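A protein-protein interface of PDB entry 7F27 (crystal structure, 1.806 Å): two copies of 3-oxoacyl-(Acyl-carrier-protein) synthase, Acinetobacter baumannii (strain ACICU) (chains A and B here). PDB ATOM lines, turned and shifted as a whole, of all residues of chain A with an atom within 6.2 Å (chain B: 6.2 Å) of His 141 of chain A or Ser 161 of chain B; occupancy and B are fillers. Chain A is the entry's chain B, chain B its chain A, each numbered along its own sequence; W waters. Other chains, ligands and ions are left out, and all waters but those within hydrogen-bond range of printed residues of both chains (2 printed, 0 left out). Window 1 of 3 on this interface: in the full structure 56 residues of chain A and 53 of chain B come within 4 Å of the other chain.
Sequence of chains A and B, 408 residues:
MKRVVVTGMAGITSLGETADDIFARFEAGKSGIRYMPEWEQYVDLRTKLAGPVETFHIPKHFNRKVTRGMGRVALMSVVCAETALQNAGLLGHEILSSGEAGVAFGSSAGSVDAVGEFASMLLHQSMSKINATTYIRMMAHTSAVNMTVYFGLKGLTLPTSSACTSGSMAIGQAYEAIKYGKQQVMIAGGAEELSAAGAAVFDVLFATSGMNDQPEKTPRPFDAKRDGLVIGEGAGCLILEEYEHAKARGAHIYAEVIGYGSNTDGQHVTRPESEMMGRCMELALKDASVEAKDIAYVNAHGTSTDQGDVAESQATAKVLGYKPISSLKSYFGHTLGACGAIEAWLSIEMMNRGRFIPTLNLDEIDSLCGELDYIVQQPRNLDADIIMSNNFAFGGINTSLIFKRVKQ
Of the printed residues of chain B, Tyr 135 of chain A touches Ser 108, Ala 163 and Phe 394. Printed residues of chain B within 4 Å of His 141 of chain A: Ser 161 (3.9 Å), Ser 162 (3.6 Å) and Ala 163 (3.8 Å). Of the printed residues of chain B, Pro 159 of chain A touches Pro 159, Ser 161 and Met 169. Printed residues of chain A within 4 Å of Ser 108 of chain B: Tyr 135. Printed residues of chain A within 4 Å of Ser 161 of chain B: His 141 (3.9 Å) and Pro 159 (3.7 Å). The nearest printed residue of chain A that does not touch Ser 161 of chain B is Ala 140 of chain A (6.0 Å).
Along chain A the printed residues that touch a printed residue of chain B span positions 135 to 161. Printed residues of chain B that touch a printed residue of chain A: Ser 108, Pro 159, Ser 161, Ser 162, Ala 163, Met 169, Phe 394 and Ile 397. Among the printed residues, 13 pairs touch across the chains. Among the printed residues, no Asp or Glu carboxylate lies within 4 Å of a Lys or Arg side-chain nitrogen of the other chain.
His 141 of chain A touches Ser 161 of chain B, but with the chains exchanged Ser 161 of chain A does not touch His 141 of chain B (4.1 Å). Pro 159 of chain B touches its own counterpart, Pro 159 of chain A. Pro 159 of chain A touches Ser 161 of chain B, and with the chains exchanged Ser 161 of chain A touches Pro 159 of chain B. 8 positions are printed for both chains.
OG of Ser 166 of chain B sits at hydrogen-bond distance from O of Ala 163 of chain B. OG of Ser 162 of chain B sits at hydrogen-bond distance from O of Thr 160 of chain B, 3.3 Å away. The side-chain hydroxyl of Ser 162 of chain B lies close to the side-chain sulfur of Met 169 of chain B (3.6 Å). A ring nitrogen (NE2) of His 141 of chain A lies close to the side-chain sulfur of Met 139 of chain A, at 3.6 Å. O of Ala 140 of chain A lies within hydrogen-bond range of OG of Ser 161 of chain A (2.7 Å). The backbone NH (N) of Ser 107 of chain B sits at hydrogen-bond distance from the side-chain hydroxyl (OG) of Ser 161 of chain B, at 3.1 Å.
O of Pro 159 of chain B lies close to O of Pro 159 of chain A (3.2 Å). The backbone carbonyl oxygen (O) of Ser 108 of chain B sits at hydrogen-bond distance from the side-chain hydroxyl (OH) of Tyr 135 of chain A, at 2.9 Å.
Water W1 lies within hydrogen-bond range of O of Phe 394 of chain B (2.7 Å), NE2 of His 141 of chain A (2.7 Å) and O of Ser 162 of chain B (2.8 Å). Water W2 lies within hydrogen-bond range of O of Ser 108 of chain B (2.8 Å) and N of Ala 140 of chain A (3.0 Å).
Among the printed residues, merely in contact across the chains: Pro 159 of chain A with Met 169 of chain B (3.6 Å), His 141 of chain A with Ser 162 of chain B (3.6 Å), Ser 161 of chain A with Pro 159 of chain B (3.6 Å), Pro 159 of chain A with Ser 161 of chain B (3.7 Å), Tyr 135 of chain A with Ala 163 of chain B (3.7 Å), Thr 157 of chain A with Met 169 of chain B (3.7 Å), Thr 157 of chain A with Ile 397 of chain B (3.8 Å), His 141 of chain A with Ala 163 of chain B (3.8 Å), Ile 136 of chain A with Phe 394 of chain B (3.8 Å), Tyr 135 of chain A with Phe 394 of chain B (3.8 Å) and His 141 of chain A with Ser 161 of chain B (3.9 Å).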
ATOM      1  N   PHE A 105      15.865 -10.401  -2.619  1.00  0.00           N
ATOM      2  CA  PHE A 105      15.399 -10.330  -3.994  1.00  0.00           C
ATOM      3  C   PHE A 105      16.580 -10.001  -4.889  1.00  0.00           C
ATOM      4  O   PHE A 105      17.556  -9.387  -4.449  1.00  0.00           O
ATOM      5  CB  PHE A 105      14.297  -9.275  -4.145  1.00  0.00           C
ATOM      6  CG  PHE A 105      13.144  -9.717  -5.010  1.00  0.00           C
ATOM      7  CD1 PHE A 105      13.175  -9.501  -6.382  1.00  0.00           C
ATOM      8  CD2 PHE A 105      12.044 -10.360  -4.456  1.00  0.00           C
ATOM      9  CE1 PHE A 105      12.115  -9.908  -7.189  1.00  0.00           C
ATOM     10  CE2 PHE A 105      10.973 -10.775  -5.261  1.00  0.00           C
ATOM     11  CZ  PHE A 105      11.019 -10.549  -6.627  1.00  0.00           C
ATOM     12  N   GLY A 106      16.489 -10.416  -6.145  1.00  0.00           N
ATOM     13  CA  GLY A 106      17.542 -10.037  -7.070  1.00  0.00           C
ATOM     14  C   GLY A 106      17.070 -10.114  -8.502  1.00  0.00           C
ATOM     15  O   GLY A 106      16.021 -10.682  -8.809  1.00  0.00           O
ATOM     16  N   SER A 107      17.884  -9.527  -9.379  1.00  0.00           N
ATOM     17  CA  SER A 107      17.690  -9.594 -10.819  1.00  0.00           C
ATOM     18  C   SER A 107      19.066  -9.567 -11.467  1.00  0.00           C
ATOM     19  O   SER A 107      20.064  -9.226 -10.823  1.00  0.00           O
ATOM     20  CB  SER A 107      16.807  -8.440 -11.324  1.00  0.00           C
ATOM     21  OG  SER A 107      17.334  -7.180 -10.949  1.00  0.00           O
ATOM     22  N   GLY A 110      19.083  -4.030 -13.499  1.00  0.00           N
ATOM     23  CA  GLY A 110      17.955  -3.141 -13.322  1.00  0.00           C
ATOM     24  C   GLY A 110      17.227  -2.891 -14.628  1.00  0.00           C
ATOM     25  O   GLY A 110      17.308  -3.672 -15.582  1.00  0.00           O
ATOM     26  N   TYR A 135      19.324   6.128 -10.936  1.00  0.00           N
ATOM     27  CA  TYR A 135      20.061   5.074 -10.245  1.00  0.00           C
ATOM     28  C   TYR A 135      19.103   4.084  -9.588  1.00  0.00           C
ATOM     29  O   TYR A 135      19.291   2.868  -9.720  1.00  0.00           O
ATOM     30  CB  TYR A 135      21.065   5.655  -9.229  1.00  0.00           C
ATOM     31  CG  TYR A 135      21.925   4.551  -8.621  1.00  0.00           C
ATOM     32  CD1 TYR A 135      22.712   3.723  -9.427  1.00  0.00           C
ATOM     33  CD2 TYR A 135      21.932   4.322  -7.255  1.00  0.00           C
ATOM     34  CE1 TYR A 135      23.462   2.676  -8.881  1.00  0.00           C
ATOM     35  CE2 TYR A 135      22.665   3.258  -6.695  1.00  0.00           C
ATOM     36  CZ  TYR A 135      23.434   2.455  -7.513  1.00  0.00           C
ATOM     37  OH  TYR A 135      24.163   1.420  -6.951  1.00  0.00           O
ATOM     38  N   ILE A 136      18.045   4.581  -8.926  1.00  0.00           N
ATOM     39  CA  ILE A 136      17.072   3.689  -8.285  1.00  0.00           C
ATOM     40  C   ILE A 136      16.481   2.716  -9.289  1.00  0.00           C
ATOM     41  O   ILE A 136      16.281   1.530  -8.987  1.00  0.00           O
ATOM     42  CB  ILE A 136      15.971   4.483  -7.559  1.00  0.00           C
ATOM     43  CG1 ILE A 136      16.575   5.576  -6.679  1.00  0.00           C
ATOM     44  CG2 ILE A 136      15.112   3.530  -6.731  1.00  0.00           C
ATOM     45  CD1 ILE A 136      17.514   5.063  -5.580  1.00  0.00           C
ATOM     46  N   MET A 138      17.892   1.862 -12.305  1.00  0.00           N
ATOM     47  CA  MET A 138      18.888   1.083 -13.033  1.00  0.00           C
ATOM     48  C   MET A 138      19.599   0.041 -12.176  1.00  0.00           C
ATOM     49  O   MET A 138      20.094  -0.955 -12.715  1.00  0.00           O
ATOM     50  CB  MET A 138      19.946   2.012 -13.644  1.00  0.00           C
ATOM     51  CG  MET A 138      20.979   2.533 -12.645  1.00  0.00           C
ATOM     52  SD  MET A 138      22.444   3.296 -13.410  1.00  0.00           S
ATOM     53  CE  MET A 138      23.021   1.971 -14.463  1.00  0.00           C
ATOM     54  N   MET A 139      19.681   0.255 -10.868  1.00  0.00           N
ATOM     55  CA  MET A 139      20.590  -0.525 -10.042  1.00  0.00           C
ATOM     56  C   MET A 139      20.048  -1.941  -9.874  1.00  0.00           C
ATOM     57  O   MET A 139      18.831  -2.169  -9.924  1.00  0.00           O
ATOM     58  CB  MET A 139      20.781   0.172  -8.690  1.00  0.00           C
ATOM     59  CG  MET A 139      19.617  -0.071  -7.751  1.00  0.00           C
ATOM     60  SD  MET A 139      19.408   0.979  -6.337  1.00  0.00           S
ATOM     61  CE  MET A 139      19.554   2.615  -6.790  1.00  0.00           C
ATOM     62  N   ALA A 140      20.976  -2.910  -9.772  1.00  0.00           N
ATOM     63  CA  ALA A 140      20.583  -4.316  -9.788  1.00  0.00           C
ATOM     64  C   ALA A 140      19.734  -4.724  -8.581  1.00  0.00           C
ATOM     65  O   ALA A 140      19.043  -5.747  -8.648  1.00  0.00           O
ATOM     66  CB  ALA A 140      21.809  -5.220  -9.890  1.00  0.00           C
ATOM     67  N   HIS A 141      19.746  -3.959  -7.486  1.00  0.00           N
ATOM     68  CA  HIS A 141      18.834  -4.219  -6.373  1.00  0.00           C
ATOM     69  C   HIS A 141      17.609  -3.300  -6.394  1.00  0.00           C
ATOM     70  O   HIS A 141      17.007  -3.029  -5.348  1.00  0.00           O
ATOM     71  CB  HIS A 141      19.556  -4.155  -5.019  1.00  0.00           C
ATOM     72  CG  HIS A 141      20.282  -2.874  -4.740  1.00  0.00           C
ATOM     73  ND1 HIS A 141      21.158  -2.289  -5.634  1.00  0.00           N
ATOM     74  CD2 HIS A 141      20.311  -2.099  -3.627  1.00  0.00           C
ATOM     75  CE1 HIS A 141      21.661  -1.189  -5.099  1.00  0.00           C
ATOM     76  NE2 HIS A 141      21.164  -1.052  -3.881  1.00  0.00           N
ATOM     77  N   THR A 142      17.188  -2.867  -7.588  1.00  0.00           N
ATOM     78  CA  THR A 142      16.021  -1.988  -7.681  1.00  0.00           C
ATOM     79  C   THR A 142      14.774  -2.647  -7.103  1.00  0.00           C
ATOM     80  O   THR A 142      13.966  -1.969  -6.456  1.00  0.00           O
ATOM     81  CB  THR A 142      15.783  -1.552  -9.142  1.00  0.00           C
ATOM     82  OG1 THR A 142      14.711  -0.608  -9.182  1.00  0.00           O
ATOM     83  CG2 THR A 142      15.474  -2.737 -10.071  1.00  0.00           C
ATOM     84  N   SER A 143      14.625  -3.967  -7.268  1.00  0.00           N
ATOM     85  CA  SER A 143      13.413  -4.637  -6.802  1.00  0.00           C
ATOM     86  C   SER A 143      13.348  -4.656  -5.283  1.00  0.00           C
ATOM     87  O   SER A 143      12.305  -4.345  -4.690  1.00  0.00           O
ATOM     88  CB  SER A 143      13.348  -6.064  -7.336  1.00  0.00           C
ATOM     89  OG  SER A 143      13.041  -6.086  -8.712  1.00  0.00           O
ATOM     90  N   ALA A 144      14.451  -5.043  -4.634  1.00  0.00           N
ATOM     91  CA  ALA A 144      14.429  -5.163  -3.182  1.00  0.00           C
ATOM     92  C   ALA A 144      14.187  -3.808  -2.536  1.00  0.00           C
ATOM     93  O   ALA A 144      13.374  -3.690  -1.611  1.00  0.00           O
ATOM     94  CB  ALA A 144      15.734  -5.798  -2.690  1.00  0.00           C
ATOM     95  N   VAL A 145      14.867  -2.766  -3.026  1.00  0.00           N
ATOM     96  CA  VAL A 145      14.709  -1.440  -2.431  1.00  0.00           C
ATOM     97  C   VAL A 145      13.286  -0.927  -2.640  1.00  0.00           C
ATOM     98  O   VAL A 145      12.659  -0.391  -1.716  1.00  0.00           O
ATOM     99  CB  VAL A 145      15.755  -0.468  -3.002  1.00  0.00           C
ATOM    100  CG1 VAL A 145      15.364   0.964  -2.694  1.00  0.00           C
ATOM    101  CG2 VAL A 145      17.139  -0.812  -2.425  1.00  0.00           C
ATOM    102  N   ASN A 146      12.755  -1.077  -3.852  1.00  0.00           N
ATOM    103  CA  ASN A 146      11.387  -0.612  -4.082  1.00  0.00           C
ATOM    104  C   ASN A 146      10.396  -1.353  -3.198  1.00  0.00           C
ATOM    105  O   ASN A 146       9.383  -0.776  -2.779  1.00  0.00           O
ATOM    106  CB  ASN A 146      11.016  -0.750  -5.559  1.00  0.00           C
ATOM    107  CG  ASN A 146      11.384   0.493  -6.358  1.00  0.00           C
ATOM    108  OD1 ASN A 146      10.830   1.571  -6.130  1.00  0.00           O
ATOM    109  ND2 ASN A 146      12.356   0.362  -7.260  1.00  0.00           N
ATOM    110  N   THR A 157      17.349  -6.191   4.336  1.00  0.00           N
ATOM    111  CA  THR A 157      17.365  -6.177   2.871  1.00  0.00           C
ATOM    112  C   THR A 157      18.550  -7.026   2.423  1.00  0.00           C
ATOM    113  O   THR A 157      19.711  -6.669   2.681  1.00  0.00           O
ATOM    114  CB  THR A 157      17.497  -4.762   2.301  1.00  0.00           C
ATOM    115  OG1 THR A 157      16.403  -3.947   2.725  1.00  0.00           O
ATOM    116  CG2 THR A 157      17.510  -4.801   0.787  1.00  0.00           C
ATOM    117  N   PRO A 159      20.184  -8.230  -0.915  1.00  0.00           N
ATOM    118  CA  PRO A 159      20.196  -8.159  -2.382  1.00  0.00           C
ATOM    119  C   PRO A 159      20.918  -9.377  -2.938  1.00  0.00           C
ATOM    120  O   PRO A 159      22.116  -9.556  -2.715  1.00  0.00           O
ATOM    121  CB  PRO A 159      20.963  -6.858  -2.657  1.00  0.00           C
ATOM    122  CG  PRO A 159      21.968  -6.778  -1.507  1.00  0.00           C
ATOM    123  CD  PRO A 159      21.267  -7.434  -0.301  1.00  0.00           C
ATOM    124  N   SER A 161      21.170 -10.276  -6.196  1.00  0.00           N
ATOM    125  CA  SER A 161      21.409 -10.154  -7.625  1.00  0.00           C
ATOM    126  C   SER A 161      22.665 -10.937  -8.005  1.00  0.00           C
ATOM    127  O   SER A 161      23.787 -10.530  -7.688  1.00  0.00           O
ATOM    128  CB  SER A 161      21.511  -8.673  -8.006  1.00  0.00           C
ATOM    129  OG  SER A 161      20.230  -8.054  -7.825  1.00  0.00           O
ATOM    130  N   PHE B 105      31.467  -9.787  -1.724  1.00  0.00           N
ATOM    131  CA  PHE B 105      31.978  -8.560  -2.317  1.00  0.00           C
ATOM    132  C   PHE B 105      30.863  -7.851  -3.054  1.00  0.00           C
ATOM    133  O   PHE B 105      29.915  -8.486  -3.530  1.00  0.00           O
ATOM    134  CB  PHE B 105      33.139  -8.852  -3.283  1.00  0.00           C
ATOM    135  CG  PHE B 105      34.288  -7.906  -3.146  1.00  0.00           C
ATOM    136  CD1 PHE B 105      34.319  -6.717  -3.871  1.00  0.00           C
ATOM    137  CD2 PHE B 105      35.330  -8.189  -2.288  1.00  0.00           C
ATOM    138  CE1 PHE B 105      35.387  -5.843  -3.758  1.00  0.00           C
ATOM    139  CE2 PHE B 105      36.401  -7.306  -2.160  1.00  0.00           C
ATOM    140  CZ  PHE B 105      36.417  -6.126  -2.892  1.00  0.00           C
ATOM    141  N   GLY B 106      30.993  -6.528  -3.162  1.00  0.00           N
ATOM    142  CA  GLY B 106      30.006  -5.775  -3.914  1.00  0.00           C
ATOM    143  C   GLY B 106      30.527  -4.421  -4.342  1.00  0.00           C
ATOM    144  O   GLY B 106      31.569  -3.942  -3.879  1.00  0.00           O
ATOM    145  N   SER B 107      29.764  -3.809  -5.246  1.00  0.00           N
ATOM    146  CA  SER B 107      30.001  -2.456  -5.731  1.00  0.00           C
ATOM    147  C   SER B 107      28.658  -1.860  -6.143  1.00  0.00           C
ATOM    148  O   SER B 107      27.694  -2.587  -6.387  1.00  0.00           O
ATOM    149  CB  SER B 107      30.985  -2.457  -6.909  1.00  0.00           C
ATOM    150  OG  SER B 107      30.495  -3.251  -7.973  1.00  0.00           O
ATOM    151  N   SER B 108      28.597  -0.526  -6.230  1.00  0.00           N
ATOM    152  CA  SER B 108      27.349   0.109  -6.672  1.00  0.00           C
ATOM    153  C   SER B 108      27.012  -0.258  -8.108  1.00  0.00           C
ATOM    154  O   SER B 108      25.827  -0.345  -8.472  1.00  0.00           O
ATOM    155  CB  SER B 108      27.435   1.629  -6.558  1.00  0.00           C
ATOM    156  OG  SER B 108      27.604   2.040  -5.220  1.00  0.00           O
ATOM    157  N   ALA B 109      28.032  -0.463  -8.933  1.00  0.00           N
ATOM    158  CA  ALA B 109      27.846  -0.776 -10.339  1.00  0.00           C
ATOM    159  C   ALA B 109      29.091  -1.498 -10.833  1.00  0.00           C
ATOM    160  O   ALA B 109      30.147  -1.453 -10.194  1.00  0.00           O
ATOM    161  CB  ALA B 109      27.584   0.494 -11.157  1.00  0.00           C
ATOM    162  N   ALA B 140      26.863  -6.098 -11.591  1.00  0.00           N
ATOM    163  CA  ALA B 140      27.199  -5.519 -10.297  1.00  0.00           C
ATOM    164  C   ALA B 140      27.994  -6.472  -9.416  1.00  0.00           C
ATOM    165  O   ALA B 140      28.627  -6.010  -8.461  1.00  0.00           O
ATOM    166  CB  ALA B 140      25.933  -5.070  -9.560  1.00  0.00           C
ATOM    167  N   HIS B 141      27.960  -7.783  -9.686  1.00  0.00           N
ATOM    168  CA  HIS B 141      28.797  -8.739  -8.962  1.00  0.00           C
ATOM    169  C   HIS B 141      30.038  -9.138  -9.760  1.00  0.00           C
ATOM    170  O   HIS B 141      30.548 -10.255  -9.618  1.00  0.00           O
ATOM    171  CB  HIS B 141      27.997  -9.973  -8.513  1.00  0.00           C
ATOM    172  CG  HIS B 141      27.379 -10.786  -9.610  1.00  0.00           C
ATOM    173  ND1 HIS B 141      26.594 -10.240 -10.606  1.00  0.00           N
ATOM    174  CD2 HIS B 141      27.363 -12.128  -9.814  1.00  0.00           C
ATOM    175  CE1 HIS B 141      26.153 -11.206 -11.395  1.00  0.00           C
ATOM    176  NE2 HIS B 141      26.611 -12.360 -10.940  1.00  0.00           N
ATOM    177  N   THR B 142      30.548  -8.217 -10.582  1.00  0.00           N
ATOM    178  CA  THR B 142      31.747  -8.487 -11.368  1.00  0.00           C
ATOM    179  C   THR B 142      32.972  -8.739 -10.483  1.00  0.00           C
ATOM    180  O   THR B 142      33.811  -9.582 -10.810  1.00  0.00           O
ATOM    181  CB  THR B 142      31.996  -7.329 -12.342  1.00  0.00           C
ATOM    182  OG1 THR B 142      33.131  -7.627 -13.163  1.00  0.00           O
ATOM    183  CG2 THR B 142      32.268  -6.027 -11.609  1.00  0.00           C
ATOM    184  N   LEU B 158      28.979 -14.639  -2.238  1.00  0.00           N
ATOM    185  CA  LEU B 158      27.947 -13.791  -1.634  1.00  0.00           C
ATOM    186  C   LEU B 158      28.000 -12.411  -2.256  1.00  0.00           C
ATOM    187  O   LEU B 158      28.813 -11.564  -1.836  1.00  0.00           O
ATOM    188  CB  LEU B 158      28.114 -13.703  -0.120  1.00  0.00           C
ATOM    189  CG  LEU B 158      28.087 -15.038   0.621  1.00  0.00           C
ATOM    190  CD1 LEU B 158      28.380 -14.781   2.090  1.00  0.00           C
ATOM    191  CD2 LEU B 158      26.752 -15.752   0.428  1.00  0.00           C
ATOM    192  N   PRO B 159      27.165 -12.131  -3.260  1.00  0.00           N
ATOM    193  CA  PRO B 159      27.163 -10.798  -3.881  1.00  0.00           C
ATOM    194  C   PRO B 159      26.430  -9.826  -2.968  1.00  0.00           C
ATOM    195  O   PRO B 159      25.263 -10.030  -2.631  1.00  0.00           O
ATOM    196  CB  PRO B 159      26.406 -11.022  -5.197  1.00  0.00           C
ATOM    197  CG  PRO B 159      25.451 -12.161  -4.872  1.00  0.00           C
ATOM    198  CD  PRO B 159      26.169 -13.041  -3.861  1.00  0.00           C
ATOM    199  N   THR B 160      27.124  -8.793  -2.529  1.00  0.00           N
ATOM    200  CA  THR B 160      26.548  -7.837  -1.595  1.00  0.00           C
ATOM    201  C   THR B 160      26.524  -6.442  -2.195  1.00  0.00           C
ATOM    202  O   THR B 160      26.740  -5.440  -1.508  1.00  0.00           O
ATOM    203  CB  THR B 160      27.305  -7.833  -0.272  1.00  0.00           C
ATOM    204  OG1 THR B 160      28.673  -7.536  -0.538  1.00  0.00           O
ATOM    205  CG2 THR B 160      27.225  -9.201   0.390  1.00  0.00           C
ATOM    206  N   SER B 161      26.236  -6.360  -3.487  1.00  0.00           N
ATOM    207  CA  SER B 161      26.129  -5.066  -4.148  1.00  0.00           C
ATOM    208  C   SER B 161      24.878  -4.350  -3.656  1.00  0.00           C
ATOM    209  O   SER B 161      23.758  -4.734  -3.998  1.00  0.00           O
ATOM    210  CB  SER B 161      26.121  -5.271  -5.658  1.00  0.00           C
ATOM    211  OG  SER B 161      27.423  -5.690  -6.073  1.00  0.00           O
ATOM    212  N   SER B 162      25.067  -3.316  -2.839  1.00  0.00           N
ATOM    213  CA  SER B 162      23.980  -2.600  -2.181  1.00  0.00           C
ATOM    214  C   SER B 162      24.328  -1.120  -2.074  1.00  0.00           C
ATOM    215  O   SER B 162      24.102  -0.481  -1.039  1.00  0.00           O
ATOM    216  CB  SER B 162      23.679  -3.200  -0.802  1.00  0.00           C
ATOM    217  OG  SER B 162      24.846  -3.244   0.029  1.00  0.00           O
ATOM    218  N   ALA B 163      24.901  -0.571  -3.145  1.00  0.00           N
ATOM    219  CA  ALA B 163      25.355   0.831  -3.220  1.00  0.00           C
ATOM    220  C   ALA B 163      26.335   1.088  -2.071  1.00  0.00           C
ATOM    221  O   ALA B 163      27.325   0.347  -1.942  1.00  0.00           O
ATOM    222  CB  ALA B 163      24.133   1.757  -3.275  1.00  0.00           C
ATOM    223  N   SER B 166      27.888  -1.760   0.225  1.00  0.00           N
ATOM    224  CA  SER B 166      28.356  -2.993  -0.405  1.00  0.00           C
ATOM    225  C   SER B 166      29.482  -3.639   0.394  1.00  0.00           C
ATOM    226  O   SER B 166      29.472  -4.853   0.646  1.00  0.00           O
ATOM    227  CB  SER B 166      28.824  -2.713  -1.835  1.00  0.00           C
ATOM    228  OG  SER B 166      27.737  -2.354  -2.676  1.00  0.00           O
ATOM    229  N   MET B 169      28.301  -4.604   4.167  1.00  0.00           N
ATOM    230  CA  MET B 169      27.465  -5.791   4.056  1.00  0.00           C
ATOM    231  C   MET B 169      28.295  -7.011   3.679  1.00  0.00           C
ATOM    232  O   MET B 169      28.031  -8.110   4.177  1.00  0.00           O
ATOM    233  CB  MET B 169      26.327  -5.550   3.045  1.00  0.00           C
ATOM    234  CG  MET B 169      25.373  -6.713   2.849  1.00  0.00           C
ATOM    235  SD  MET B 169      24.128  -6.382   1.558  1.00  0.00           S
ATOM    236  CE  MET B 169      23.103  -5.142   2.359  1.00  0.00           C
ATOM    237  N   PHE B 394      21.438   4.052  -0.091  1.00  0.00           N
ATOM    238  CA  PHE B 394      20.153   4.212  -0.758  1.00  0.00           C
ATOM    239  C   PHE B 394      19.252   3.027  -0.469  1.00  0.00           C
ATOM    240  O   PHE B 394      19.713   1.907  -0.225  1.00  0.00           O
ATOM    241  CB  PHE B 394      20.341   4.367  -2.274  1.00  0.00           C
ATOM    242  CG  PHE B 394      20.749   5.748  -2.684  1.00  0.00           C
ATOM    243  CD1 PHE B 394      20.980   6.716  -1.721  1.00  0.00           C
ATOM    244  CD2 PHE B 394      20.864   6.091  -4.017  1.00  0.00           C
ATOM    245  CE1 PHE B 394      21.352   8.000  -2.078  1.00  0.00           C
ATOM    246  CE2 PHE B 394      21.239   7.378  -4.389  1.00  0.00           C
ATOM    247  CZ  PHE B 394      21.482   8.335  -3.417  1.00  0.00           C
ATOM    248  N   ILE B 397      19.216   1.218   3.467  1.00  0.00           N
ATOM    249  CA  ILE B 397      19.924   0.037   3.953  1.00  0.00           C
ATOM    250  C   ILE B 397      21.007   0.491   4.924  1.00  0.00           C
ATOM    251  O   ILE B 397      21.827   1.355   4.595  1.00  0.00           O
ATOM    252  CB  ILE B 397      20.527  -0.764   2.787  1.00  0.00           C
ATOM    253  CG1 ILE B 397      19.433  -1.211   1.805  1.00  0.00           C
ATOM    254  CG2 ILE B 397      21.302  -1.992   3.317  1.00  0.00           C
ATOM    255  CD1 ILE B 397      20.003  -1.996   0.631  1.00  0.00           C
HETATM  256  O   HOH W   1      21.559   0.422  -1.600  1.00  0.00           O
HETATM  257  O   HOH W   2      23.885  -2.012  -9.668  1.00  0.00           O
